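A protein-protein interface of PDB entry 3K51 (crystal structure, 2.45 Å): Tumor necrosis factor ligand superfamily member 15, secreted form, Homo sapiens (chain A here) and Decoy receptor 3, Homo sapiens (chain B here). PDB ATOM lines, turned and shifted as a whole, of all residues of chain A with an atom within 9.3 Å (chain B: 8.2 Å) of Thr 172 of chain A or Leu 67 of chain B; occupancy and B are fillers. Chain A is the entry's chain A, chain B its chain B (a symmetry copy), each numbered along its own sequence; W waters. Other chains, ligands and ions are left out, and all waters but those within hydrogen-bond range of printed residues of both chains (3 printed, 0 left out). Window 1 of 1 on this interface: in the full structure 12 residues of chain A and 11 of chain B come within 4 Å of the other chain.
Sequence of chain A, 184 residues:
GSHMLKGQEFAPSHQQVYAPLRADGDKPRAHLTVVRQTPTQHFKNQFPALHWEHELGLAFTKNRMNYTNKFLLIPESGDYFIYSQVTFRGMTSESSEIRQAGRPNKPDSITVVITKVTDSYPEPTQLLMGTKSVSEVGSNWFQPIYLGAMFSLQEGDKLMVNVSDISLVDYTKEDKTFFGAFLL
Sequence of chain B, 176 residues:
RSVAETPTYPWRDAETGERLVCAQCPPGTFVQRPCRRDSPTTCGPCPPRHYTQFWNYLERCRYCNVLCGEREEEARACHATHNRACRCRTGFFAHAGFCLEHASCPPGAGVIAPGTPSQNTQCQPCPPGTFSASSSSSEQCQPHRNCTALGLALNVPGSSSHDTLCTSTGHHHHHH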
ATOM      1  N   THR A  33      11.342 -10.269  18.507  1.00  0.00           N
ATOM      2  CA  THR A  33      12.209 -10.863  17.506  1.00  0.00           C
ATOM      3  C   THR A  33      13.148  -9.831  16.887  1.00  0.00           C
ATOM      4  O   THR A  33      12.865  -8.638  16.892  1.00  0.00           O
ATOM      5  CB  THR A  33      11.400 -11.544  16.401  1.00  0.00           C
ATOM      6  OG1 THR A  33      10.504 -10.596  15.815  1.00  0.00           O
ATOM      7  CG2 THR A  33      10.594 -12.707  16.971  1.00  0.00           C
ATOM      8  N   VAL A  34      14.260 -10.312  16.344  1.00  0.00           N
ATOM      9  CA  VAL A  34      15.311  -9.448  15.827  1.00  0.00           C
ATOM     10  C   VAL A  34      14.861  -8.674  14.580  1.00  0.00           C
ATOM     11  O   VAL A  34      14.088  -9.186  13.764  1.00  0.00           O
ATOM     12  CB  VAL A  34      16.586 -10.266  15.508  1.00  0.00           C
ATOM     13  CG1 VAL A  34      16.385 -11.120  14.247  1.00  0.00           C
ATOM     14  CG2 VAL A  34      17.817  -9.345  15.379  1.00  0.00           C
ATOM     15  N   VAL A  35      15.302  -7.423  14.475  1.00  0.00           N
ATOM     16  CA  VAL A  35      15.224  -6.671  13.215  1.00  0.00           C
ATOM     17  C   VAL A  35      16.623  -6.241  12.794  1.00  0.00           C
ATOM     18  O   VAL A  35      17.601  -6.514  13.496  1.00  0.00           O
ATOM     19  CB  VAL A  35      14.341  -5.410  13.339  1.00  0.00           C
ATOM     20  CG1 VAL A  35      12.900  -5.788  13.642  1.00  0.00           C
ATOM     21  CG2 VAL A  35      14.895  -4.467  14.399  1.00  0.00           C
ATOM     22  N   ARG A  36      16.724  -5.568  11.653  1.00  0.00           N
ATOM     23  CA  ARG A  36      17.998  -5.005  11.227  1.00  0.00           C
ATOM     24  C   ARG A  36      18.433  -3.925  12.206  1.00  0.00           C
ATOM     25  O   ARG A  36      17.687  -2.984  12.473  1.00  0.00           O
ATOM     26  CB  ARG A  36      17.896  -4.428   9.810  1.00  0.00           C
ATOM     27  CG  ARG A  36      19.243  -4.147   9.162  1.00  0.00           C
ATOM     28  CD  ARG A  36      19.083  -3.440   7.819  1.00  0.00           C
ATOM     29  NE  ARG A  36      18.368  -4.259   6.841  1.00  0.00           N
ATOM     30  CZ  ARG A  36      18.935  -5.213   6.105  1.00  0.00           C
ATOM     31  NH1 ARG A  36      20.228  -5.476   6.241  1.00  0.00           N
ATOM     32  NH2 ARG A  36      18.207  -5.908   5.236  1.00  0.00           N
ATOM     33  N   GLN A  37      19.633  -4.077  12.757  1.00  0.00           N
ATOM     34  CA  GLN A  37      20.167  -3.107  13.716  1.00  0.00           C
ATOM     35  C   GLN A  37      20.801  -1.919  12.995  1.00  0.00           C
ATOM     36  O   GLN A  37      21.425  -2.078  11.946  1.00  0.00           O
ATOM     37  CB  GLN A  37      21.193  -3.772  14.642  1.00  0.00           C
ATOM     38  CG  GLN A  37      20.697  -5.059  15.319  1.00  0.00           C
ATOM     39  CD  GLN A  37      19.479  -4.828  16.204  1.00  0.00           C
ATOM     40  OE1 GLN A  37      19.495  -3.974  17.097  1.00  0.00           O
ATOM     41  NE2 GLN A  37      18.415  -5.586  15.959  1.00  0.00           N
ATOM     42  N   GLU A  53      11.564  -6.222  17.031  1.00  0.00           N
ATOM     43  CA  GLU A  53      10.185  -6.197  16.553  1.00  0.00           C
ATOM     44  C   GLU A  53       9.252  -6.649  17.684  1.00  0.00           C
ATOM     45  O   GLU A  53       9.583  -7.560  18.442  1.00  0.00           O
ATOM     46  CB  GLU A  53      10.035  -7.131  15.343  1.00  0.00           C
ATOM     47  CG  GLU A  53       8.607  -7.283  14.838  1.00  0.00           C
ATOM     48  CD  GLU A  53       8.026  -5.977  14.339  1.00  0.00           C
ATOM     49  OE1 GLU A  53       8.647  -5.347  13.460  1.00  0.00           O
ATOM     50  OE2 GLU A  53       6.945  -5.580  14.826  1.00  0.00           O
ATOM     51  N   THR A  87      21.949 -15.198  17.906  1.00  0.00           N
ATOM     52  CA  THR A  87      22.831 -15.928  17.011  1.00  0.00           C
ATOM     53  C   THR A  87      23.907 -14.997  16.472  1.00  0.00           C
ATOM     54  O   THR A  87      23.610 -13.938  15.904  1.00  0.00           O
ATOM     55  CB  THR A  87      22.063 -16.591  15.846  1.00  0.00           C
ATOM     56  OG1 THR A  87      21.118 -17.535  16.371  1.00  0.00           O
ATOM     57  CG2 THR A  87      23.025 -17.320  14.924  1.00  0.00           C
ATOM     58  N   ARG A  89      27.241 -14.360  13.996  1.00  0.00           N
ATOM     59  CA  ARG A  89      27.851 -14.824  12.756  1.00  0.00           C
ATOM     60  C   ARG A  89      29.047 -13.961  12.374  1.00  0.00           C
ATOM     61  O   ARG A  89      28.994 -12.732  12.449  1.00  0.00           O
ATOM     62  CB  ARG A  89      26.826 -14.851  11.615  1.00  0.00           C
ATOM     63  CG  ARG A  89      26.147 -13.516  11.349  1.00  0.00           C
ATOM     64  CD  ARG A  89      25.473 -13.499   9.989  1.00  0.00           C
ATOM     65  NE  ARG A  89      24.800 -12.229   9.731  1.00  0.00           N
ATOM     66  CZ  ARG A  89      25.412 -11.048   9.718  1.00  0.00           C
ATOM     67  NH1 ARG A  89      24.724  -9.945   9.470  1.00  0.00           N
ATOM     68  NH2 ARG A  89      26.713 -10.971   9.963  1.00  0.00           N
ATOM     69  N   LEU A 168      27.957  -8.457  14.530  1.00  0.00           N
ATOM     70  CA  LEU A 168      28.071  -9.911  14.445  1.00  0.00           C
ATOM     71  C   LEU A 168      26.709 -10.607  14.582  1.00  0.00           C
ATOM     72  O   LEU A 168      26.600 -11.812  14.387  1.00  0.00           O
ATOM     73  CB  LEU A 168      29.040 -10.432  15.512  1.00  0.00           C
ATOM     74  CG  LEU A 168      30.519 -10.040  15.367  1.00  0.00           C
ATOM     75  CD1 LEU A 168      31.341 -10.600  16.519  1.00  0.00           C
ATOM     76  CD2 LEU A 168      31.084 -10.513  14.030  1.00  0.00           C
ATOM     77  N   VAL A 169      25.676  -9.835  14.906  1.00  0.00           N
ATOM     78  CA  VAL A 169      24.358 -10.395  15.193  1.00  0.00           C
ATOM     79  C   VAL A 169      23.609 -10.779  13.921  1.00  0.00           C
ATOM     80  O   VAL A 169      23.313  -9.928  13.080  1.00  0.00           O
ATOM     81  CB  VAL A 169      23.488  -9.411  16.018  1.00  0.00           C
ATOM     82  CG1 VAL A 169      22.059  -9.925  16.136  1.00  0.00           C
ATOM     83  CG2 VAL A 169      24.093  -9.193  17.392  1.00  0.00           C
ATOM     84  N   ASP A 170      23.300 -12.066  13.791  1.00  0.00           N
ATOM     85  CA  ASP A 170      22.418 -12.537  12.735  1.00  0.00           C
ATOM     86  C   ASP A 170      21.010 -11.969  12.926  1.00  0.00           C
ATOM     87  O   ASP A 170      20.328 -12.297  13.894  1.00  0.00           O
ATOM     88  CB  ASP A 170      22.370 -14.061  12.735  1.00  0.00           C
ATOM     89  CG  ASP A 170      21.778 -14.627  11.459  1.00  0.00           C
ATOM     90  OD1 ASP A 170      21.071 -13.892  10.741  1.00  0.00           O
ATOM     91  OD2 ASP A 170      22.028 -15.814  11.170  1.00  0.00           O
ATOM     92  N   TYR A 171      20.582 -11.130  11.985  1.00  0.00           N
ATOM     93  CA  TYR A 171      19.305 -10.437  12.078  1.00  0.00           C
ATOM     94  C   TYR A 171      18.353 -10.893  10.976  1.00  0.00           C
ATOM     95  O   TYR A 171      17.282 -10.316  10.794  1.00  0.00           O
ATOM     96  CB  TYR A 171      19.522  -8.925  11.962  1.00  0.00           C
ATOM     97  CG  TYR A 171      20.219  -8.528  10.687  1.00  0.00           C
ATOM     98  CD1 TYR A 171      19.529  -8.485   9.483  1.00  0.00           C
ATOM     99  CD2 TYR A 171      21.579  -8.240  10.675  1.00  0.00           C
ATOM    100  CE1 TYR A 171      20.167  -8.149   8.308  1.00  0.00           C
ATOM    101  CE2 TYR A 171      22.226  -7.902   9.507  1.00  0.00           C
ATOM    102  CZ  TYR A 171      21.515  -7.856   8.324  1.00  0.00           C
ATOM    103  OH  TYR A 171      22.154  -7.525   7.155  1.00  0.00           O
ATOM    104  N   THR A 172      18.743 -11.932  10.246  1.00  0.00           N
ATOM    105  CA  THR A 172      18.073 -12.266   8.986  1.00  0.00           C
ATOM    106  C   THR A 172      16.722 -12.981   9.154  1.00  0.00           C
ATOM    107  O   THR A 172      15.912 -13.010   8.224  1.00  0.00           O
ATOM    108  CB  THR A 172      18.988 -13.090   8.053  1.00  0.00           C
ATOM    109  OG1 THR A 172      19.434 -14.271   8.730  1.00  0.00           O
ATOM    110  CG2 THR A 172      20.204 -12.256   7.619  1.00  0.00           C
ATOM    111  N   LYS A 173      16.480 -13.558  10.328  1.00  0.00           N
ATOM    112  CA  LYS A 173      15.199 -14.219  10.577  1.00  0.00           C
ATOM    113  C   LYS A 173      14.774 -14.221  12.041  1.00  0.00           C
ATOM    114  O   LYS A 173      15.611 -14.297  12.946  1.00  0.00           O
ATOM    115  CB  LYS A 173      15.191 -15.638  10.007  1.00  0.00           C
ATOM    116  CG  LYS A 173      13.789 -16.147   9.679  1.00  0.00           C
ATOM    117  CD  LYS A 173      13.818 -17.437   8.876  1.00  0.00           C
ATOM    118  CE  LYS A 173      12.421 -18.058   8.796  1.00  0.00           C
ATOM    119  NZ  LYS A 173      12.376 -19.250   7.901  1.00  0.00           N
ATOM    120  N   GLU A 174      13.461 -14.157  12.260  1.00  0.00           N
ATOM    121  CA  GLU A 174      12.887 -14.035  13.607  1.00  0.00           C
ATOM    122  C   GLU A 174      13.146 -15.256  14.506  1.00  0.00           C
ATOM    123  O   GLU A 174      13.059 -15.157  15.727  1.00  0.00           O
ATOM    124  CB  GLU A 174      11.378 -13.748  13.525  1.00  0.00           C
ATOM    125  CG  GLU A 174      10.570 -14.847  12.829  1.00  0.00           C
ATOM    126  CD  GLU A 174       9.098 -14.477  12.633  1.00  0.00           C
ATOM    127  OE1 GLU A 174       8.595 -13.570  13.348  1.00  0.00           O
ATOM    128  OE2 GLU A 174       8.442 -15.106  11.771  1.00  0.00           O
ATOM    129  N   ASP A 175      13.460 -16.401  13.906  1.00  0.00           N
ATOM    130  CA  ASP A 175      13.630 -17.635  14.687  1.00  0.00           C
ATOM    131  C   ASP A 175      15.040 -17.832  15.279  1.00  0.00           C
ATOM    132  O   ASP A 175      15.261 -18.757  16.057  1.00  0.00           O
ATOM    133  CB  ASP A 175      13.201 -18.868  13.876  1.00  0.00           C
ATOM    134  CG  ASP A 175      13.965 -19.007  12.555  1.00  0.00           C
ATOM    135  OD1 ASP A 175      14.542 -18.007  12.085  1.00  0.00           O
ATOM    136  OD2 ASP A 175      13.973 -20.120  11.985  1.00  0.00           O
ATOM    137  N   LYS A 176      15.976 -16.952  14.926  1.00  0.00           N
ATOM    138  CA  LYS A 176      17.380 -17.124  15.327  1.00  0.00           C
ATOM    139  C   LYS A 176      17.815 -16.189  16.457  1.00  0.00           C
ATOM    140  O   LYS A 176      18.705 -16.526  17.251  1.00  0.00           O
ATOM    141  CB  LYS A 176      18.312 -16.964  14.121  1.00  0.00           C
ATOM    142  CG  LYS A 176      18.466 -18.236  13.295  1.00  0.00           C
ATOM    143  CD  LYS A 176      19.474 -18.061  12.178  1.00  0.00           C
ATOM    144  CE  LYS A 176      18.960 -17.103  11.122  1.00  0.00           C
ATOM    145  NZ  LYS A 176      19.815 -17.116   9.900  1.00  0.00           N
ATOM    146  N   THR A 177      17.198 -15.014  16.521  1.00  0.00           N
ATOM    147  CA  THR A 177      17.536 -14.027  17.526  1.00  0.00           C
ATOM    148  C   THR A 177      16.252 -13.425  18.095  1.00  0.00           C
ATOM    149  O   THR A 177      15.439 -12.880  17.358  1.00  0.00           O
ATOM    150  CB  THR A 177      18.447 -12.913  16.932  1.00  0.00           C
ATOM    151  OG1 THR A 177      19.676 -13.494  16.477  1.00  0.00           O
ATOM    152  CG2 THR A 177      18.756 -11.837  17.975  1.00  0.00           C
ATOM    153  N   ARG B  49       3.575  -6.000   3.689  1.00  0.00           N
ATOM    154  CA  ARG B  49       4.604  -6.822   4.330  1.00  0.00           C
ATOM    155  C   ARG B  49       4.064  -8.174   4.813  1.00  0.00           C
ATOM    156  O   ARG B  49       4.720  -8.884   5.584  1.00  0.00           O
ATOM    157  CB  ARG B  49       5.293  -6.055   5.464  1.00  0.00           C
ATOM    158  CG  ARG B  49       6.154  -4.882   4.982  1.00  0.00           C
ATOM    159  CD  ARG B  49       6.640  -4.022   6.144  1.00  0.00           C
ATOM    160  NE  ARG B  49       7.734  -4.654   6.878  1.00  0.00           N
ATOM    161  CZ  ARG B  49       8.012  -4.417   8.156  1.00  0.00           C
ATOM    162  NH1 ARG B  49       7.266  -3.573   8.856  1.00  0.00           N
ATOM    163  NH2 ARG B  49       9.025  -5.037   8.739  1.00  0.00           N
ATOM    164  N   TYR B  63       3.794 -13.223   7.751  1.00  0.00           N
ATOM    165  CA  TYR B  63       4.643 -12.043   7.713  1.00  0.00           C
ATOM    166  C   TYR B  63       5.856 -12.296   6.832  1.00  0.00           C
ATOM    167  O   TYR B  63       6.487 -13.345   6.927  1.00  0.00           O
ATOM    168  CB  TYR B  63       5.093 -11.690   9.136  1.00  0.00           C
ATOM    169  CG  TYR B  63       6.102 -10.566   9.223  1.00  0.00           C
ATOM    170  CD1 TYR B  63       5.857  -9.333   8.621  1.00  0.00           C
ATOM    171  CD2 TYR B  63       7.285 -10.726   9.934  1.00  0.00           C
ATOM    172  CE1 TYR B  63       6.772  -8.301   8.706  1.00  0.00           C
ATOM    173  CE2 TYR B  63       8.206  -9.697  10.034  1.00  0.00           C
ATOM    174  CZ  TYR B  63       7.944  -8.487   9.414  1.00  0.00           C
ATOM    175  OH  TYR B  63       8.853  -7.462   9.508  1.00  0.00           O
ATOM    176  N   CYS B  64       6.177 -11.334   5.971  1.00  0.00           N
ATOM    177  CA  CYS B  64       7.403 -11.405   5.174  1.00  0.00           C
ATOM    178  C   CYS B  64       8.622 -11.282   6.092  1.00  0.00           C
ATOM    179  O   CYS B  64       9.105 -10.183   6.368  1.00  0.00           O
ATOM    180  CB  CYS B  64       7.410 -10.316   4.080  1.00  0.00           C
ATOM    181  SG  CYS B  64       6.189 -10.606   2.710  1.00  0.00           S
ATOM    182  N   ASN B  65       9.093 -12.423   6.583  1.00  0.00           N
ATOM    183  CA  ASN B  65      10.024 -12.456   7.710  1.00  0.00           C
ATOM    184  C   ASN B  65      11.476 -12.723   7.313  1.00  0.00           C
ATOM    185  O   ASN B  65      12.329 -12.947   8.172  1.00  0.00           O
ATOM    186  CB  ASN B  65       9.572 -13.499   8.733  1.00  0.00           C
ATOM    187  CG  ASN B  65       9.457 -14.891   8.135  1.00  0.00           C
ATOM    188  OD1 ASN B  65       9.641 -15.078   6.931  1.00  0.00           O
ATOM    189  ND2 ASN B  65       9.159 -15.874   8.974  1.00  0.00           N
ATOM    190  N   VAL B  66      11.750 -12.717   6.015  1.00  0.00           N
ATOM    191  CA  VAL B  66      13.111 -12.926   5.532  1.00  0.00           C
ATOM    192  C   VAL B  66      13.789 -11.596   5.215  1.00  0.00           C
ATOM    193  O   VAL B  66      13.312 -10.828   4.378  1.00  0.00           O
ATOM    194  CB  VAL B  66      13.141 -13.830   4.279  1.00  0.00           C
ATOM    195  CG1 VAL B  66      14.529 -13.848   3.671  1.00  0.00           C
ATOM    196  CG2 VAL B  66      12.697 -15.243   4.633  1.00  0.00           C
ATOM    197  N   LEU B  67      14.882 -11.316   5.911  1.00  0.00           N
ATOM    198  CA  LEU B  67      15.703 -10.155   5.599  1.00  0.00           C
ATOM    199  C   LEU B  67      16.976 -10.601   4.895  1.00  0.00           C
ATOM    200  O   LEU B  67      17.622 -11.566   5.311  1.00  0.00           O
ATOM    201  CB  LEU B  67      16.049  -9.372   6.875  1.00  0.00           C
ATOM    202  CG  LEU B  67      14.887  -8.690   7.613  1.00  0.00           C
ATOM    203  CD1 LEU B  67      15.280  -8.331   9.040  1.00  0.00           C
ATOM    204  CD2 LEU B  67      14.407  -7.457   6.863  1.00  0.00           C
ATOM    205  N   CYS B  68      17.332  -9.905   3.836  1.00  0.00           N
ATOM    206  CA  CYS B  68      18.548 -10.225   3.129  1.00  0.00           C
ATOM    207  C   CYS B  68      19.705  -9.556   3.847  1.00  0.00           C
ATOM    208  O   CYS B  68      19.616  -8.408   4.245  1.00  0.00           O
ATOM    209  CB  CYS B  68      18.414  -9.854   1.655  1.00  0.00           C
ATOM    210  SG  CYS B  68      17.196 -10.920   0.825  1.00  0.00           S
ATOM    211  N   GLY B  69      20.771 -10.305   4.056  1.00  0.00           N
ATOM    212  CA  GLY B  69      21.870  -9.824   4.858  1.00  0.00           C
ATOM    213  C   GLY B  69      23.248 -10.161   4.353  1.00  0.00           C
ATOM    214  O   GLY B  69      23.410 -11.010   3.503  1.00  0.00           O
ATOM    215  N   GLU B  70      24.254  -9.474   4.867  1.00  0.00           N
ATOM    216  CA  GLU B  70      25.609  -9.798   4.491  1.00  0.00           C
ATOM    217  C   GLU B  70      25.736  -9.645   2.999  1.00  0.00           C
ATOM    218  O   GLU B  70      25.430  -8.592   2.453  1.00  0.00           O
ATOM    219  CB  GLU B  70      25.953 -11.222   4.921  1.00  0.00           C
ATOM    220  CG  GLU B  70      25.392 -12.326   4.038  1.00  0.00           C
ATOM    221  CD  GLU B  70      25.233 -13.649   4.777  1.00  0.00           C
ATOM    222  OE1 GLU B  70      24.403 -14.469   4.361  1.00  0.00           O
ATOM    223  OE2 GLU B  70      25.944 -13.877   5.767  1.00  0.00           O
ATOM    224  N   ARG B  71      26.209 -10.690   2.337  1.00  0.00           N
ATOM    225  CA  ARG B  71      26.382 -10.644   0.903  1.00  0.00           C
ATOM    226  C   ARG B  71      25.172 -11.236   0.197  1.00  0.00           C
ATOM    227  O   ARG B  71      25.264 -12.307  -0.402  1.00  0.00           O
ATOM    228  CB  ARG B  71      27.665 -11.383   0.528  1.00  0.00           C
ATOM    229  CG  ARG B  71      28.894 -10.894   1.290  1.00  0.00           C
ATOM    230  CD  ARG B  71      29.365  -9.526   0.795  1.00  0.00           C
ATOM    231  NE  ARG B  71      30.350  -8.918   1.691  1.00  0.00           N
ATOM    232  CZ  ARG B  71      31.182  -7.937   1.348  1.00  0.00           C
ATOM    233  NH1 ARG B  71      31.167  -7.443   0.118  1.00  0.00           N
ATOM    234  NH2 ARG B  71      32.036  -7.452   2.237  1.00  0.00           N
ATOM    235  N   GLU B  72      24.037 -10.554   0.274  1.00  0.00           N
ATOM    236  CA  GLU B  72      22.823 -11.048  -0.348  1.00  0.00           C
ATOM    237  C   GLU B  72      21.990  -9.915  -0.894  1.00  0.00           C
ATOM    238  O   GLU B  72      22.066  -8.800  -0.404  1.00  0.00           O
ATOM    239  CB  GLU B  72      21.981 -11.810   0.668  1.00  0.00           C
ATOM    240  CG  GLU B  72      22.505 -13.163   1.096  1.00  0.00           C
ATOM    241  CD  GLU B  72      21.603 -13.829   2.122  1.00  0.00           C
ATOM    242  OE1 GLU B  72      20.631 -13.202   2.571  1.00  0.00           O
ATOM    243  OE2 GLU B  72      21.866 -14.984   2.486  1.00  0.00           O
ATOM    244  N   GLU B  73      21.181 -10.216  -1.901  1.00  0.00           N
ATOM    245  CA  GLU B  73      20.195  -9.279  -2.428  1.00  0.00           C
ATOM    246  C   GLU B  73      18.855  -9.977  -2.637  1.00  0.00           C
ATOM    247  O   GLU B  73      18.772 -11.208  -2.597  1.00  0.00           O
ATOM    248  CB  GLU B  73      20.680  -8.647  -3.744  1.00  0.00           C
ATOM    249  CG  GLU B  73      20.546  -9.551  -4.974  1.00  0.00           C
ATOM    250  CD  GLU B  73      21.892  -9.927  -5.585  1.00  0.00           C
ATOM    251  OE1 GLU B  73      22.785  -9.054  -5.646  1.00  0.00           O
ATOM    252  OE2 GLU B  73      22.047 -11.090  -6.022  1.00  0.00           O
ATOM    253  N   GLU B  74      17.807  -9.189  -2.856  1.00  0.00           N
ATOM    254  CA  GLU B  74      16.482  -9.739  -3.087  1.00  0.00           C
ATOM    255  C   GLU B  74      16.417 -10.511  -4.397  1.00  0.00           C
ATOM    256  O   GLU B  74      16.721  -9.973  -5.461  1.00  0.00           O
ATOM    257  CB  GLU B  74      15.431  -8.630  -3.088  1.00  0.00           C
ATOM    258  CG  GLU B  74      15.088  -8.096  -1.714  1.00  0.00           C
ATOM    259  CD  GLU B  74      13.800  -7.296  -1.710  1.00  0.00           C
ATOM    260  OE1 GLU B  74      13.085  -7.309  -2.735  1.00  0.00           O
ATOM    261  OE2 GLU B  74      13.504  -6.650  -0.680  1.00  0.00           O
ATOM    262  N   ASN B  83       6.401 -14.685   0.001  1.00  0.00           N
ATOM    263  CA  ASN B  83       7.410 -14.145   0.899  1.00  0.00           C
ATOM    264  C   ASN B  83       8.532 -13.459   0.128  1.00  0.00           C
ATOM    265  O   ASN B  83       8.705 -13.685  -1.069  1.00  0.00           O
ATOM    266  CB  ASN B  83       7.995 -15.273   1.767  1.00  0.00           C
ATOM    267  CG  ASN B  83       8.662 -14.758   3.031  1.00  0.00           C
ATOM    268  OD1 ASN B  83       8.807 -13.547   3.227  1.00  0.00           O
ATOM    269  ND2 ASN B  83       9.067 -15.674   3.900  1.00  0.00           N
ATOM    270  N   ARG B  84       9.286 -12.613   0.822  1.00  0.00           N
ATOM    271  CA  ARG B  84      10.542 -12.106   0.300  1.00  0.00           C
ATOM    272  C   ARG B  84      11.545 -13.251   0.223  1.00  0.00           C
ATOM    273  O   ARG B  84      11.483 -14.191   1.012  1.00  0.00           O
ATOM    274  CB  ARG B  84      11.073 -10.997   1.211  1.00  0.00           C
ATOM    275  CG  ARG B  84      12.211 -10.177   0.621  1.00  0.00           C
ATOM    276  CD  ARG B  84      12.359  -8.836   1.342  1.00  0.00           C
ATOM    277  NE  ARG B  84      12.216  -8.975   2.786  1.00  0.00           N
ATOM    278  CZ  ARG B  84      11.284  -8.365   3.511  1.00  0.00           C
ATOM    279  NH1 ARG B  84      10.418  -7.546   2.930  1.00  0.00           N
ATOM    280  NH2 ARG B  84      11.231  -8.557   4.824  1.00  0.00           N
ATOM    281  N   ALA B  85      12.452 -13.185  -0.743  1.00  0.00           N
ATOM    282  CA  ALA B  85      13.493 -14.198  -0.874  1.00  0.00           C
ATOM    283  C   ALA B  85      14.840 -13.560  -1.177  1.00  0.00           C
ATOM    284  O   ALA B  85      14.908 -12.492  -1.787  1.00  0.00           O
ATOM    285  CB  ALA B  85      13.122 -15.207  -1.949  1.00  0.00           C
ATOM    286  N   CYS B  86      15.912 -14.215  -0.745  1.00  0.00           N
ATOM    287  CA  CYS B  86      17.251 -13.675  -0.921  1.00  0.00           C
ATOM    288  C   CYS B  86      18.174 -14.679  -1.600  1.00  0.00           C
ATOM    289  O   CYS B  86      18.072 -15.884  -1.378  1.00  0.00           O
ATOM    290  CB  CYS B  86      17.843 -13.243   0.426  1.00  0.00           C
ATOM    291  SG  CYS B  86      16.792 -12.116   1.390  1.00  0.00           S
ATOM    292  N   GLY B  97      24.648 -23.056   4.822  1.00  0.00           N
ATOM    293  CA  GLY B  97      24.129 -21.977   5.654  1.00  0.00           C
ATOM    294  C   GLY B  97      24.947 -20.704   5.567  1.00  0.00           C
ATOM    295  O   GLY B  97      24.627 -19.707   6.213  1.00  0.00           O
HETATM  296  O   HOH W   1       9.672 -17.826  11.336  1.00  0.00           O
HETATM  297  O   HOH W   2      11.731 -11.683  10.729  1.00  0.00           O
HETATM  298  O   HOH W   3       9.796 -17.752   6.780  1.00  0.00           O
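The backbone carbonyl oxygen (O) of Thr 172 of chain A sits at hydrogen-bond distance from the backbone NH (N) of Leu 67 of chain B (3.0 Å).
O of Cys 68 of chain B sits at hydrogen-bond distance from NH2 of Arg 36 of chain A, 3.0 Å away.
The side-chain carboxylate (OE2) of Glu 174 of chain A is in hydrogen-bond range of the side-chain amide nitrogen (ND2) of Asn 65 of chain B (3.0 Å).
The side-chain sulfur (SG) of Cys 68 of chain B is disulfide-bonded to the side-chain sulfur (SG) of Cys 86 of chain B.
The side-chain amide oxygen of Asn 65 of chain B is in hydrogen-bond range of the side-chain amide nitrogen of Asn 83 of chain B (3.1 Å).
OG1 of Thr 172 of chain A is in hydrogen-bond range of OD1 of Asp 170 of chain A, 2.6 Å away.
The backbone carbonyl oxygen (O) of Val 66 of chain B lies within hydrogen-bond range of the guanidinium group (NE) of Arg 84 of chain B.
The side-chain hydroxyl (OG1) of Thr 172 of chain A lies within hydrogen-bond range of the side-chain amino group (NZ) of Lys 176 of chain A (3.1 Å).
The guanidinium group (NH1) of Arg 36 of chain A is in hydrogen-bond range of the side-chain hydroxyl (OH) of Tyr 171 of chain A (3.0 Å).
Tyr 171 of chain A touches Leu 67 of chain B.
Tyr 171 of chain A touches Cys 68 of chain B (OH to O, 3.96 Å).
Tyr 171 of chain A touches Gly 69 of chain B.
Glu 70 of chain B touches Tyr 171 of chain A (N to OH, 3.7 Å).
Thr 172 of chain A touches Asn 65 of chain B.
Val 66 of chain B touches Thr 172 of chain A.
CG of Lys 173 of chain A touches O of Asn 65 of chain B, 3.8 Å away.
Leu 67 of chain B touches just these residues of chain A: Tyr 171 and Thr 172.
Val 66 of chain B touches just one residue of chain A: Thr 172.
Of the printed residues of chain B, Tyr 171 of chain A touches Leu 67, Cys 68, Gly 69 and Glu 70.
Of the printed residues of chain A, Gly 69 of chain B touches Tyr 171 (3.3 Å).
Of the printed residues of chain B, Lys 173 of chain A touches Asn 65.
The nearest residue of chain A that does not touch Leu 67 of chain B is Arg 36 of chain A (4.1 Å).
Of the 18 printed residues of chain A, 5 touch a printed residue of chain B.
Printed residues of chain B that touch a printed residue of chain A: Asn 65, Val 66, Leu 67, Cys 68, Gly 69 and Glu 70.
Among the printed residues, 10 pairs touch across the chains.
Among the printed residues, no Asp or Glu carboxylate lies within 4 Å of a Lys or Arg side-chain nitrogen of the other chain.
Water W3 bridges the side-chain amide oxygen of Asn 65 of chain B (2.7 Å) and the side-chain amino group of Lys 173 of chain A (3.2 Å).
Water W2 bridges the backbone carbonyl oxygen (O) of Asn 65 of chain B (2.9 Å) and the backbone NH (N) of Glu 174 of chain A (3.4 Å).
Water W1 lies within hydrogen-bond range of OE2 of Glu 174 of chain A and ND2 of Asn 65 of chain B.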
